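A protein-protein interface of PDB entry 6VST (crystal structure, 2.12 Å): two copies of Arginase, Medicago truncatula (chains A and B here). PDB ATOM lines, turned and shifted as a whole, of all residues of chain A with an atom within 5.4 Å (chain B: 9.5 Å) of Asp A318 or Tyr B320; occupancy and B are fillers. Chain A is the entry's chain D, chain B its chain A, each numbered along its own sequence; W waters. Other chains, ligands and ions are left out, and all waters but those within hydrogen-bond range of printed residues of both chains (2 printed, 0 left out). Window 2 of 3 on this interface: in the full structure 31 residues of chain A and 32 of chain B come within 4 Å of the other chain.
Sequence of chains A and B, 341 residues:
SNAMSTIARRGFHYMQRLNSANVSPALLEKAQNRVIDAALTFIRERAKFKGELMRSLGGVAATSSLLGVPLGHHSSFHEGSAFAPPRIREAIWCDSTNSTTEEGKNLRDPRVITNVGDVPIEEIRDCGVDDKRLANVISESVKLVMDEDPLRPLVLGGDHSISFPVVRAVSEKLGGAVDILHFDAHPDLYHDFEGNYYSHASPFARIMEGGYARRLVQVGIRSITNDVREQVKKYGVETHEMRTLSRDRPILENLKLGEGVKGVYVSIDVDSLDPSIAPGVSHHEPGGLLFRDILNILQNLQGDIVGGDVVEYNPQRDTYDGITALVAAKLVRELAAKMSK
Tyr B320 touches Gln A316 (CE1 to O, 3.98 Å). Asp A318 touches Tyr B320 (O to CE2, 3.7 Å). Tyr A320 touches Gln B316. Tyr A320 touches Arg B317 (OH to CG, 3.4 Å).
Water W2 lies within hydrogen-bond range of the backbone carbonyl oxygen of Arg B317 (2.7 Å) and the side-chain hydroxyl of Tyr A320 (2.7 Å). Water W1 bridges the side-chain hydroxyl (OH) of Tyr B320 (3.1 Å) and the guanidinium group (NH1) of Arg A317 (3.3 Å).
OG1 of Thr A324 lies within hydrogen-bond range of OD1 of Asp A318, at 2.7 Å. The side-chain amide oxygen (OD1) of Asn A314 is in hydrogen-bond range of the backbone NH (N) of Gln A316 (3.0 Å). The side-chain hydroxyl (OH) of Tyr A313 sits at hydrogen-bond distance from the side-chain carboxylate (OD2) of Asp A318 (3.3 Å). The side-chain carboxylate (OD2) of Asp A318 sits at hydrogen-bond distance from the backbone NH (N) of Ala A325 (3.3 Å).
NE2 of Gln A316 lies close to NH1 of Arg B87, 3.3 Å away. OH of Tyr B320 sits close to O of Arg A317, 3.4 Å away.
Gln A316 touches Tyr B320, and with the chains exchanged Tyr A320 touches Gln B316. Arg A317 touches Tyr B320, and with the chains exchanged Tyr A320 touches Arg B317. Asp A318 touches Tyr B320, but with the chains exchanged Tyr A320 does not touch Asp B318 (4.02 Å). 14 positions are printed for both chains.
Hydrophobic or aromatic side chains of chain B that line the printed part of chain A: Tyr B320. Hydrophobic or aromatic side chains of chain A that line the printed part of chain B: Tyr A320. Along chain A the printed residues that touch a printed residue of chain B span positions 316 to 320. Among the printed residues, no Asp or Glu carboxylate lies within 4 Å of a Lys or Arg side-chain nitrogen of the other chain.
No residue of chain B comes within 4 Å of Pro A279. No residue of chain B comes within 4 Å of Gly A280. Asn A314 touches none of the printed residues of chain B. Printed residues of chain B within 4 Å of Gln A316: Arg B87 and Tyr B320. Of the printed residues of chain B, Arg A317 touches Tyr B320 (3.4 Å). Printed residues of chain B within 4 Å of Asp A318: Tyr B320 (3.7 Å). Thr A319 touches none of the printed residues of chain B. Printed residues of chain B within 4 Å of Tyr A320: Gln B316 and Arg B317. No residue of chain B comes within 4 Å of Thr A324. Of the printed residues of chain A, Arg B87 touches Gln A316. Of the printed residues of chain A, Gln B316 touches Tyr A320. The nearest printed residue of chain A that does not touch Tyr B320 is Thr A319 (5.3 Å). The nearest printed residue of chain B that does not touch Tyr A320 is Asp B318 (4.02 Å).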
ATOM      1  N   PRO A 279      15.432   3.337 -32.387  1.00  0.00           N
ATOM      2  CA  PRO A 279      16.756   3.964 -32.341  1.00  0.00           C
ATOM      3  C   PRO A 279      17.881   2.970 -32.470  1.00  0.00           C
ATOM      4  O   PRO A 279      18.976   3.354 -32.903  1.00  0.00           O
ATOM      5  CB  PRO A 279      16.769   4.652 -30.967  1.00  0.00           C
ATOM      6  CG  PRO A 279      15.804   3.830 -30.135  1.00  0.00           C
ATOM      7  CD  PRO A 279      14.710   3.479 -31.107  1.00  0.00           C
ATOM      8  N   GLY A 280      17.634   1.705 -32.120  1.00  0.00           N
ATOM      9  CA  GLY A 280      18.664   0.695 -32.114  1.00  0.00           C
ATOM     10  C   GLY A 280      18.850   0.047 -33.466  1.00  0.00           C
ATOM     11  O   GLY A 280      18.576  -1.145 -33.628  1.00  0.00           O
ATOM     12  N   TYR A 313      18.332  -4.911 -36.285  1.00  0.00           N
ATOM     13  CA  TYR A 313      18.307  -4.474 -34.892  1.00  0.00           C
ATOM     14  C   TYR A 313      19.735  -4.471 -34.347  1.00  0.00           C
ATOM     15  O   TYR A 313      20.460  -5.458 -34.469  1.00  0.00           O
ATOM     16  CB  TYR A 313      17.396  -5.367 -34.038  1.00  0.00           C
ATOM     17  CG  TYR A 313      17.602  -5.178 -32.538  1.00  0.00           C
ATOM     18  CD1 TYR A 313      17.665  -3.894 -31.981  1.00  0.00           C
ATOM     19  CD2 TYR A 313      17.748  -6.274 -31.681  1.00  0.00           C
ATOM     20  CE1 TYR A 313      17.864  -3.709 -30.620  1.00  0.00           C
ATOM     21  CE2 TYR A 313      17.953  -6.093 -30.316  1.00  0.00           C
ATOM     22  CZ  TYR A 313      18.006  -4.805 -29.793  1.00  0.00           C
ATOM     23  OH  TYR A 313      18.209  -4.592 -28.448  1.00  0.00           O
ATOM     24  N   ASN A 314      20.148  -3.340 -33.775  1.00  0.00           N
ATOM     25  CA  ASN A 314      21.512  -3.116 -33.293  1.00  0.00           C
ATOM     26  C   ASN A 314      21.456  -2.823 -31.799  1.00  0.00           C
ATOM     27  O   ASN A 314      21.269  -1.667 -31.399  1.00  0.00           O
ATOM     28  CB  ASN A 314      22.166  -1.952 -34.043  1.00  0.00           C
ATOM     29  CG  ASN A 314      23.640  -1.820 -33.746  1.00  0.00           C
ATOM     30  OD1 ASN A 314      24.110  -2.233 -32.693  1.00  0.00           O
ATOM     31  ND2 ASN A 314      24.383  -1.248 -34.686  1.00  0.00           N
ATOM     32  N   PRO A 315      21.617  -3.828 -30.935  1.00  0.00           N
ATOM     33  CA  PRO A 315      21.523  -3.544 -29.490  1.00  0.00           C
ATOM     34  C   PRO A 315      22.543  -2.520 -29.010  1.00  0.00           C
ATOM     35  O   PRO A 315      22.280  -1.802 -28.035  1.00  0.00           O
ATOM     36  CB  PRO A 315      21.725  -4.919 -28.836  1.00  0.00           C
ATOM     37  CG  PRO A 315      22.186  -5.834 -29.915  1.00  0.00           C
ATOM     38  CD  PRO A 315      21.754  -5.267 -31.223  1.00  0.00           C
ATOM     39  N   GLN A 316      23.683  -2.382 -29.692  1.00  0.00           N
ATOM     40  CA  GLN A 316      24.649  -1.408 -29.214  1.00  0.00           C
ATOM     41  C   GLN A 316      24.212   0.026 -29.468  1.00  0.00           C
ATOM     42  O   GLN A 316      24.778   0.933 -28.856  1.00  0.00           O
ATOM     43  CB  GLN A 316      26.022  -1.663 -29.833  1.00  0.00           C
ATOM     44  CG  GLN A 316      26.750  -2.805 -29.166  1.00  0.00           C
ATOM     45  CD  GLN A 316      27.949  -3.251 -29.945  1.00  0.00           C
ATOM     46  OE1 GLN A 316      27.900  -3.340 -31.164  1.00  0.00           O
ATOM     47  NE2 GLN A 316      29.046  -3.526 -29.250  1.00  0.00           N
ATOM     48  N   ARG A 317      23.209   0.264 -30.308  1.00  0.00           N
ATOM     49  CA  ARG A 317      22.731   1.625 -30.538  1.00  0.00           C
ATOM     50  C   ARG A 317      21.343   1.851 -29.957  1.00  0.00           C
ATOM     51  O   ARG A 317      20.739   2.900 -30.202  1.00  0.00           O
ATOM     52  CB  ARG A 317      22.750   1.949 -32.035  1.00  0.00           C
ATOM     53  CG  ARG A 317      24.109   1.693 -32.663  1.00  0.00           C
ATOM     54  CD  ARG A 317      24.671   2.958 -33.233  1.00  0.00           C
ATOM     55  NE  ARG A 317      23.754   3.490 -34.226  1.00  0.00           N
ATOM     56  CZ  ARG A 317      23.816   4.715 -34.723  1.00  0.00           C
ATOM     57  NH1 ARG A 317      24.760   5.556 -34.318  1.00  0.00           N
ATOM     58  NH2 ARG A 317      22.925   5.090 -35.625  1.00  0.00           N
ATOM     59  N   ASP A 318      20.831   0.893 -29.187  1.00  0.00           N
ATOM     60  CA  ASP A 318      19.532   1.000 -28.534  1.00  0.00           C
ATOM     61  C   ASP A 318      19.632   1.877 -27.289  1.00  0.00           C
ATOM     62  O   ASP A 318      20.724   2.176 -26.793  1.00  0.00           O
ATOM     63  CB  ASP A 318      19.030  -0.393 -28.149  1.00  0.00           C
ATOM     64  CG  ASP A 318      17.516  -0.487 -28.096  1.00  0.00           C
ATOM     65  OD1 ASP A 318      16.837   0.539 -28.311  1.00  0.00           O
ATOM     66  OD2 ASP A 318      17.011  -1.613 -27.869  1.00  0.00           O
ATOM     67  N   THR A 319      18.477   2.279 -26.764  1.00  0.00           N
ATOM     68  CA  THR A 319      18.477   2.991 -25.494  1.00  0.00           C
ATOM     69  C   THR A 319      18.522   1.995 -24.326  1.00  0.00           C
ATOM     70  O   THR A 319      18.297   0.798 -24.499  1.00  0.00           O
ATOM     71  CB  THR A 319      17.273   3.936 -25.414  1.00  0.00           C
ATOM     72  OG1 THR A 319      16.071   3.253 -25.783  1.00  0.00           O
ATOM     73  CG2 THR A 319      17.484   5.120 -26.380  1.00  0.00           C
ATOM     74  N   TYR A 320      18.836   2.512 -23.124  1.00  0.00           N
ATOM     75  CA  TYR A 320      19.118   1.630 -21.989  1.00  0.00           C
ATOM     76  C   TYR A 320      17.909   0.784 -21.610  1.00  0.00           C
ATOM     77  O   TYR A 320      18.081  -0.296 -21.037  1.00  0.00           O
ATOM     78  CB  TYR A 320      19.617   2.459 -20.792  1.00  0.00           C
ATOM     79  CG  TYR A 320      20.082   1.734 -19.511  1.00  0.00           C
ATOM     80  CD1 TYR A 320      19.223   0.931 -18.775  1.00  0.00           C
ATOM     81  CD2 TYR A 320      21.360   1.930 -18.998  1.00  0.00           C
ATOM     82  CE1 TYR A 320      19.616   0.319 -17.587  1.00  0.00           C
ATOM     83  CE2 TYR A 320      21.766   1.316 -17.809  1.00  0.00           C
ATOM     84  CZ  TYR A 320      20.884   0.519 -17.108  1.00  0.00           C
ATOM     85  OH  TYR A 320      21.262  -0.076 -15.923  1.00  0.00           O
ATOM     86  N   ASP A 321      16.698   1.231 -21.924  1.00  0.00           N
ATOM     87  CA  ASP A 321      15.506   0.425 -21.682  1.00  0.00           C
ATOM     88  C   ASP A 321      15.343  -0.705 -22.695  1.00  0.00           C
ATOM     89  O   ASP A 321      14.493  -1.579 -22.499  1.00  0.00           O
ATOM     90  CB  ASP A 321      14.258   1.318 -21.699  1.00  0.00           C
ATOM     91  CG  ASP A 321      14.192   2.241 -22.936  1.00  0.00           C
ATOM     92  OD1 ASP A 321      14.889   1.997 -23.957  1.00  0.00           O
ATOM     93  OD2 ASP A 321      13.436   3.238 -22.880  1.00  0.00           O
ATOM     94  N   GLY A 322      16.123  -0.703 -23.769  1.00  0.00           N
ATOM     95  CA  GLY A 322      16.048  -1.786 -24.732  1.00  0.00           C
ATOM     96  C   GLY A 322      14.775  -1.759 -25.540  1.00  0.00           C
ATOM     97  O   GLY A 322      14.252  -2.822 -25.890  1.00  0.00           O
ATOM     98  N   ILE A 323      14.269  -0.561 -25.857  1.00  0.00           N
ATOM     99  CA  ILE A 323      12.982  -0.447 -26.537  1.00  0.00           C
ATOM    100  C   ILE A 323      13.020  -1.108 -27.915  1.00  0.00           C
ATOM    101  O   ILE A 323      12.017  -1.660 -28.371  1.00  0.00           O
ATOM    102  CB  ILE A 323      12.547   1.030 -26.629  1.00  0.00           C
ATOM    103  CG1 ILE A 323      11.154   1.129 -27.232  1.00  0.00           C
ATOM    104  CG2 ILE A 323      13.542   1.854 -27.468  1.00  0.00           C
ATOM    105  CD1 ILE A 323      10.150   0.249 -26.549  1.00  0.00           C
ATOM    106  N   THR A 324      14.161  -1.045 -28.612  1.00  0.00           N
ATOM    107  CA  THR A 324      14.193  -1.585 -29.966  1.00  0.00           C
ATOM    108  C   THR A 324      14.210  -3.116 -29.954  1.00  0.00           C
ATOM    109  O   THR A 324      13.754  -3.743 -30.910  1.00  0.00           O
ATOM    110  CB  THR A 324      15.389  -1.004 -30.742  1.00  0.00           C
ATOM    111  OG1 THR A 324      15.422   0.427 -30.579  1.00  0.00           O
ATOM    112  CG2 THR A 324      15.280  -1.324 -32.248  1.00  0.00           C
ATOM    113  N   ALA A 325      14.718  -3.730 -28.879  1.00  0.00           N
ATOM    114  CA  ALA A 325      14.584  -5.178 -28.698  1.00  0.00           C
ATOM    115  C   ALA A 325      13.118  -5.594 -28.646  1.00  0.00           C
ATOM    116  O   ALA A 325      12.719  -6.599 -29.246  1.00  0.00           O
ATOM    117  CB  ALA A 325      15.290  -5.615 -27.409  1.00  0.00           C
ATOM    118  N   ARG B  87      30.373  -9.774 -26.374  1.00  0.00           N
ATOM    119  CA  ARG B  87      30.733  -8.367 -26.206  1.00  0.00           C
ATOM    120  C   ARG B  87      32.171  -8.227 -25.725  1.00  0.00           C
ATOM    121  O   ARG B  87      32.908  -7.338 -26.182  1.00  0.00           O
ATOM    122  CB  ARG B  87      29.781  -7.696 -25.212  1.00  0.00           C
ATOM    123  CG  ARG B  87      28.305  -7.795 -25.572  1.00  0.00           C
ATOM    124  CD  ARG B  87      28.040  -6.952 -26.789  1.00  0.00           C
ATOM    125  NE  ARG B  87      28.693  -5.656 -26.616  1.00  0.00           N
ATOM    126  CZ  ARG B  87      28.087  -4.564 -26.152  1.00  0.00           C
ATOM    127  NH1 ARG B  87      28.782  -3.436 -26.009  1.00  0.00           N
ATOM    128  NH2 ARG B  87      26.790  -4.601 -25.857  1.00  0.00           N
ATOM    129  N   PRO B 279      30.230   0.130 -14.316  1.00  0.00           N
ATOM    130  CA  PRO B 279      28.772   0.228 -14.134  1.00  0.00           C
ATOM    131  C   PRO B 279      28.000  -0.922 -14.757  1.00  0.00           C
ATOM    132  O   PRO B 279      26.853  -1.150 -14.357  1.00  0.00           O
ATOM    133  CB  PRO B 279      28.420   1.566 -14.796  1.00  0.00           C
ATOM    134  CG  PRO B 279      29.501   1.775 -15.819  1.00  0.00           C
ATOM    135  CD  PRO B 279      30.750   1.178 -15.221  1.00  0.00           C
ATOM    136  N   GLY B 280      28.587  -1.655 -15.708  1.00  0.00           N
ATOM    137  CA  GLY B 280      27.870  -2.711 -16.391  1.00  0.00           C
ATOM    138  C   GLY B 280      27.884  -4.025 -15.631  1.00  0.00           C
ATOM    139  O   GLY B 280      28.503  -5.005 -16.056  1.00  0.00           O
ATOM    140  N   TYR B 313      29.991  -9.304 -16.020  1.00  0.00           N
ATOM    141  CA  TYR B 313      29.780  -8.193 -16.933  1.00  0.00           C
ATOM    142  C   TYR B 313      28.361  -8.283 -17.486  1.00  0.00           C
ATOM    143  O   TYR B 313      27.954  -9.320 -18.005  1.00  0.00           O
ATOM    144  CB  TYR B 313      30.804  -8.191 -18.072  1.00  0.00           C
ATOM    145  CG  TYR B 313      30.445  -7.216 -19.185  1.00  0.00           C
ATOM    146  CD1 TYR B 313      30.023  -5.916 -18.893  1.00  0.00           C
ATOM    147  CD2 TYR B 313      30.511  -7.593 -20.519  1.00  0.00           C
ATOM    148  CE1 TYR B 313      29.683  -5.041 -19.903  1.00  0.00           C
ATOM    149  CE2 TYR B 313      30.179  -6.706 -21.545  1.00  0.00           C
ATOM    150  CZ  TYR B 313      29.771  -5.435 -21.230  1.00  0.00           C
ATOM    151  OH  TYR B 313      29.429  -4.549 -22.239  1.00  0.00           O
ATOM    152  N   PRO B 315      26.055  -6.387 -20.139  1.00  0.00           N
ATOM    153  CA  PRO B 315      25.976  -5.339 -21.171  1.00  0.00           C
ATOM    154  C   PRO B 315      24.689  -4.552 -21.129  1.00  0.00           C
ATOM    155  O   PRO B 315      24.664  -3.391 -21.568  1.00  0.00           O
ATOM    156  CB  PRO B 315      26.115  -6.119 -22.490  1.00  0.00           C
ATOM    157  CG  PRO B 315      26.017  -7.573 -22.130  1.00  0.00           C
ATOM    158  CD  PRO B 315      26.401  -7.703 -20.700  1.00  0.00           C
ATOM    159  N   GLN B 316      23.616  -5.122 -20.582  1.00  0.00           N
ATOM    160  CA  GLN B 316      22.362  -4.374 -20.556  1.00  0.00           C
ATOM    161  C   GLN B 316      22.334  -3.310 -19.476  1.00  0.00           C
ATOM    162  O   GLN B 316      21.382  -2.529 -19.437  1.00  0.00           O
ATOM    163  CB  GLN B 316      21.178  -5.316 -20.374  1.00  0.00           C
ATOM    164  CG  GLN B 316      20.871  -6.142 -21.630  1.00  0.00           C
ATOM    165  CD  GLN B 316      19.882  -7.234 -21.342  1.00  0.00           C
ATOM    166  OE1 GLN B 316      20.013  -7.934 -20.355  1.00  0.00           O
ATOM    167  NE2 GLN B 316      18.878  -7.377 -22.192  1.00  0.00           N
ATOM    168  N   ARG B 317      23.347  -3.256 -18.613  1.00  0.00           N
ATOM    169  CA  ARG B 317      23.472  -2.175 -17.643  1.00  0.00           C
ATOM    170  C   ARG B 317      24.729  -1.334 -17.864  1.00  0.00           C
ATOM    171  O   ARG B 317      25.076  -0.525 -17.002  1.00  0.00           O
ATOM    172  CB  ARG B 317      23.423  -2.755 -16.226  1.00  0.00           C
ATOM    173  CG  ARG B 317      22.047  -3.358 -15.927  1.00  0.00           C
ATOM    174  CD  ARG B 317      21.977  -4.168 -14.658  1.00  0.00           C
ATOM    175  NE  ARG B 317      22.440  -3.455 -13.469  1.00  0.00           N
ATOM    176  CZ  ARG B 317      21.709  -2.615 -12.733  1.00  0.00           C
ATOM    177  NH1 ARG B 317      20.458  -2.326 -13.054  1.00  0.00           N
ATOM    178  NH2 ARG B 317      22.238  -2.063 -11.664  1.00  0.00           N
ATOM    179  N   ASP B 318      25.415  -1.503 -18.994  1.00  0.00           N
ATOM    180  CA  ASP B 318      26.595  -0.719 -19.332  1.00  0.00           C
ATOM    181  C   ASP B 318      26.194   0.645 -19.890  1.00  0.00           C
ATOM    182  O   ASP B 318      25.037   0.883 -20.251  1.00  0.00           O
ATOM    183  CB  ASP B 318      27.438  -1.460 -20.360  1.00  0.00           C
ATOM    184  CG  ASP B 318      28.906  -1.143 -20.251  1.00  0.00           C
ATOM    185  OD1 ASP B 318      29.287  -0.271 -19.434  1.00  0.00           O
ATOM    186  OD2 ASP B 318      29.679  -1.782 -20.987  1.00  0.00           O
ATOM    187  N   THR B 319      27.172   1.547 -19.986  1.00  0.00           N
ATOM    188  CA  THR B 319      26.934   2.836 -20.632  1.00  0.00           C
ATOM    189  C   THR B 319      26.770   2.652 -22.143  1.00  0.00           C
ATOM    190  O   THR B 319      27.127   1.611 -22.706  1.00  0.00           O
ATOM    191  CB  THR B 319      28.087   3.805 -20.358  1.00  0.00           C
ATOM    192  OG1 THR B 319      29.294   3.282 -20.935  1.00  0.00           O
ATOM    193  CG2 THR B 319      28.292   3.979 -18.883  1.00  0.00           C
ATOM    194  N   TYR B 320      26.233   3.684 -22.806  1.00  0.00           N
ATOM    195  CA  TYR B 320      26.047   3.577 -24.253  1.00  0.00           C
ATOM    196  C   TYR B 320      27.373   3.368 -24.978  1.00  0.00           C
ATOM    197  O   TYR B 320      27.374   2.833 -26.089  1.00  0.00           O
ATOM    198  CB  TYR B 320      25.306   4.815 -24.788  1.00  0.00           C
ATOM    199  CG  TYR B 320      24.820   4.802 -26.249  1.00  0.00           C
ATOM    200  CD1 TYR B 320      25.717   4.841 -27.313  1.00  0.00           C
ATOM    201  CD2 TYR B 320      23.460   4.820 -26.560  1.00  0.00           C
ATOM    202  CE1 TYR B 320      25.282   4.874 -28.643  1.00  0.00           C
ATOM    203  CE2 TYR B 320      23.019   4.847 -27.887  1.00  0.00           C
ATOM    204  CZ  TYR B 320      23.939   4.879 -28.921  1.00  0.00           C
ATOM    205  OH  TYR B 320      23.523   4.918 -30.240  1.00  0.00           O
ATOM    206  N   ASP B 321      28.498   3.722 -24.366  1.00  0.00           N
ATOM    207  CA  ASP B 321      29.811   3.539 -24.970  1.00  0.00           C
ATOM    208  C   ASP B 321      30.460   2.197 -24.625  1.00  0.00           C
ATOM    209  O   ASP B 321      31.554   1.910 -25.125  1.00  0.00           O
ATOM    210  CB  ASP B 321      30.732   4.689 -24.547  1.00  0.00           C
ATOM    211  CG  ASP B 321      30.599   5.034 -23.059  1.00  0.00           C
ATOM    212  OD1 ASP B 321      31.241   4.354 -22.225  1.00  0.00           O
ATOM    213  OD2 ASP B 321      29.850   5.985 -22.718  1.00  0.00           O
ATOM    214  N   GLY B 322      29.831   1.383 -23.783  1.00  0.00           N
ATOM    215  CA  GLY B 322      30.380   0.077 -23.463  1.00  0.00           C
ATOM    216  C   GLY B 322      31.685   0.110 -22.697  1.00  0.00           C
ATOM    217  O   GLY B 322      32.570  -0.714 -22.953  1.00  0.00           O
ATOM    218  N   ILE B 323      31.823   1.032 -21.743  1.00  0.00           N
ATOM    219  CA  ILE B 323      33.072   1.123 -20.995  1.00  0.00           C
ATOM    220  C   ILE B 323      33.347  -0.148 -20.182  1.00  0.00           C
ATOM    221  O   ILE B 323      34.510  -0.528 -19.987  1.00  0.00           O
ATOM    222  CB  ILE B 323      33.062   2.380 -20.104  1.00  0.00           C
ATOM    223  CG1 ILE B 323      34.464   2.635 -19.585  1.00  0.00           C
ATOM    224  CG2 ILE B 323      32.101   2.217 -18.940  1.00  0.00           C
ATOM    225  CD1 ILE B 323      35.499   2.575 -20.666  1.00  0.00           C
ATOM    226  N   THR B 324      32.304  -0.830 -19.699  1.00  0.00           N
ATOM    227  CA  THR B 324      32.543  -2.014 -18.889  1.00  0.00           C
ATOM    228  C   THR B 324      32.985  -3.203 -19.742  1.00  0.00           C
ATOM    229  O   THR B 324      33.737  -4.058 -19.261  1.00  0.00           O
ATOM    230  CB  THR B 324      31.296  -2.374 -18.078  1.00  0.00           C
ATOM    231  OG1 THR B 324      30.791  -1.207 -17.423  1.00  0.00           O
ATOM    232  CG2 THR B 324      31.629  -3.425 -17.027  1.00  0.00           C
ATOM    233  N   ALA B 325      32.534  -3.273 -20.998  1.00  0.00           N
ATOM    234  CA  ALA B 325      33.085  -4.265 -21.910  1.00  0.00           C
ATOM    235  C   ALA B 325      34.581  -4.074 -22.041  1.00  0.00           C
ATOM    236  O   ALA B 325      35.341  -5.049 -22.048  1.00  0.00           O
ATOM    237  CB  ALA B 325      32.410  -4.170 -23.282  1.00  0.00           C
HETATM  238  O   HOH W   1      25.545   6.930 -31.379  1.00  0.00           O
HETATM  239  O   HOH W   2      23.750   0.428 -14.894  1.00  0.00           O
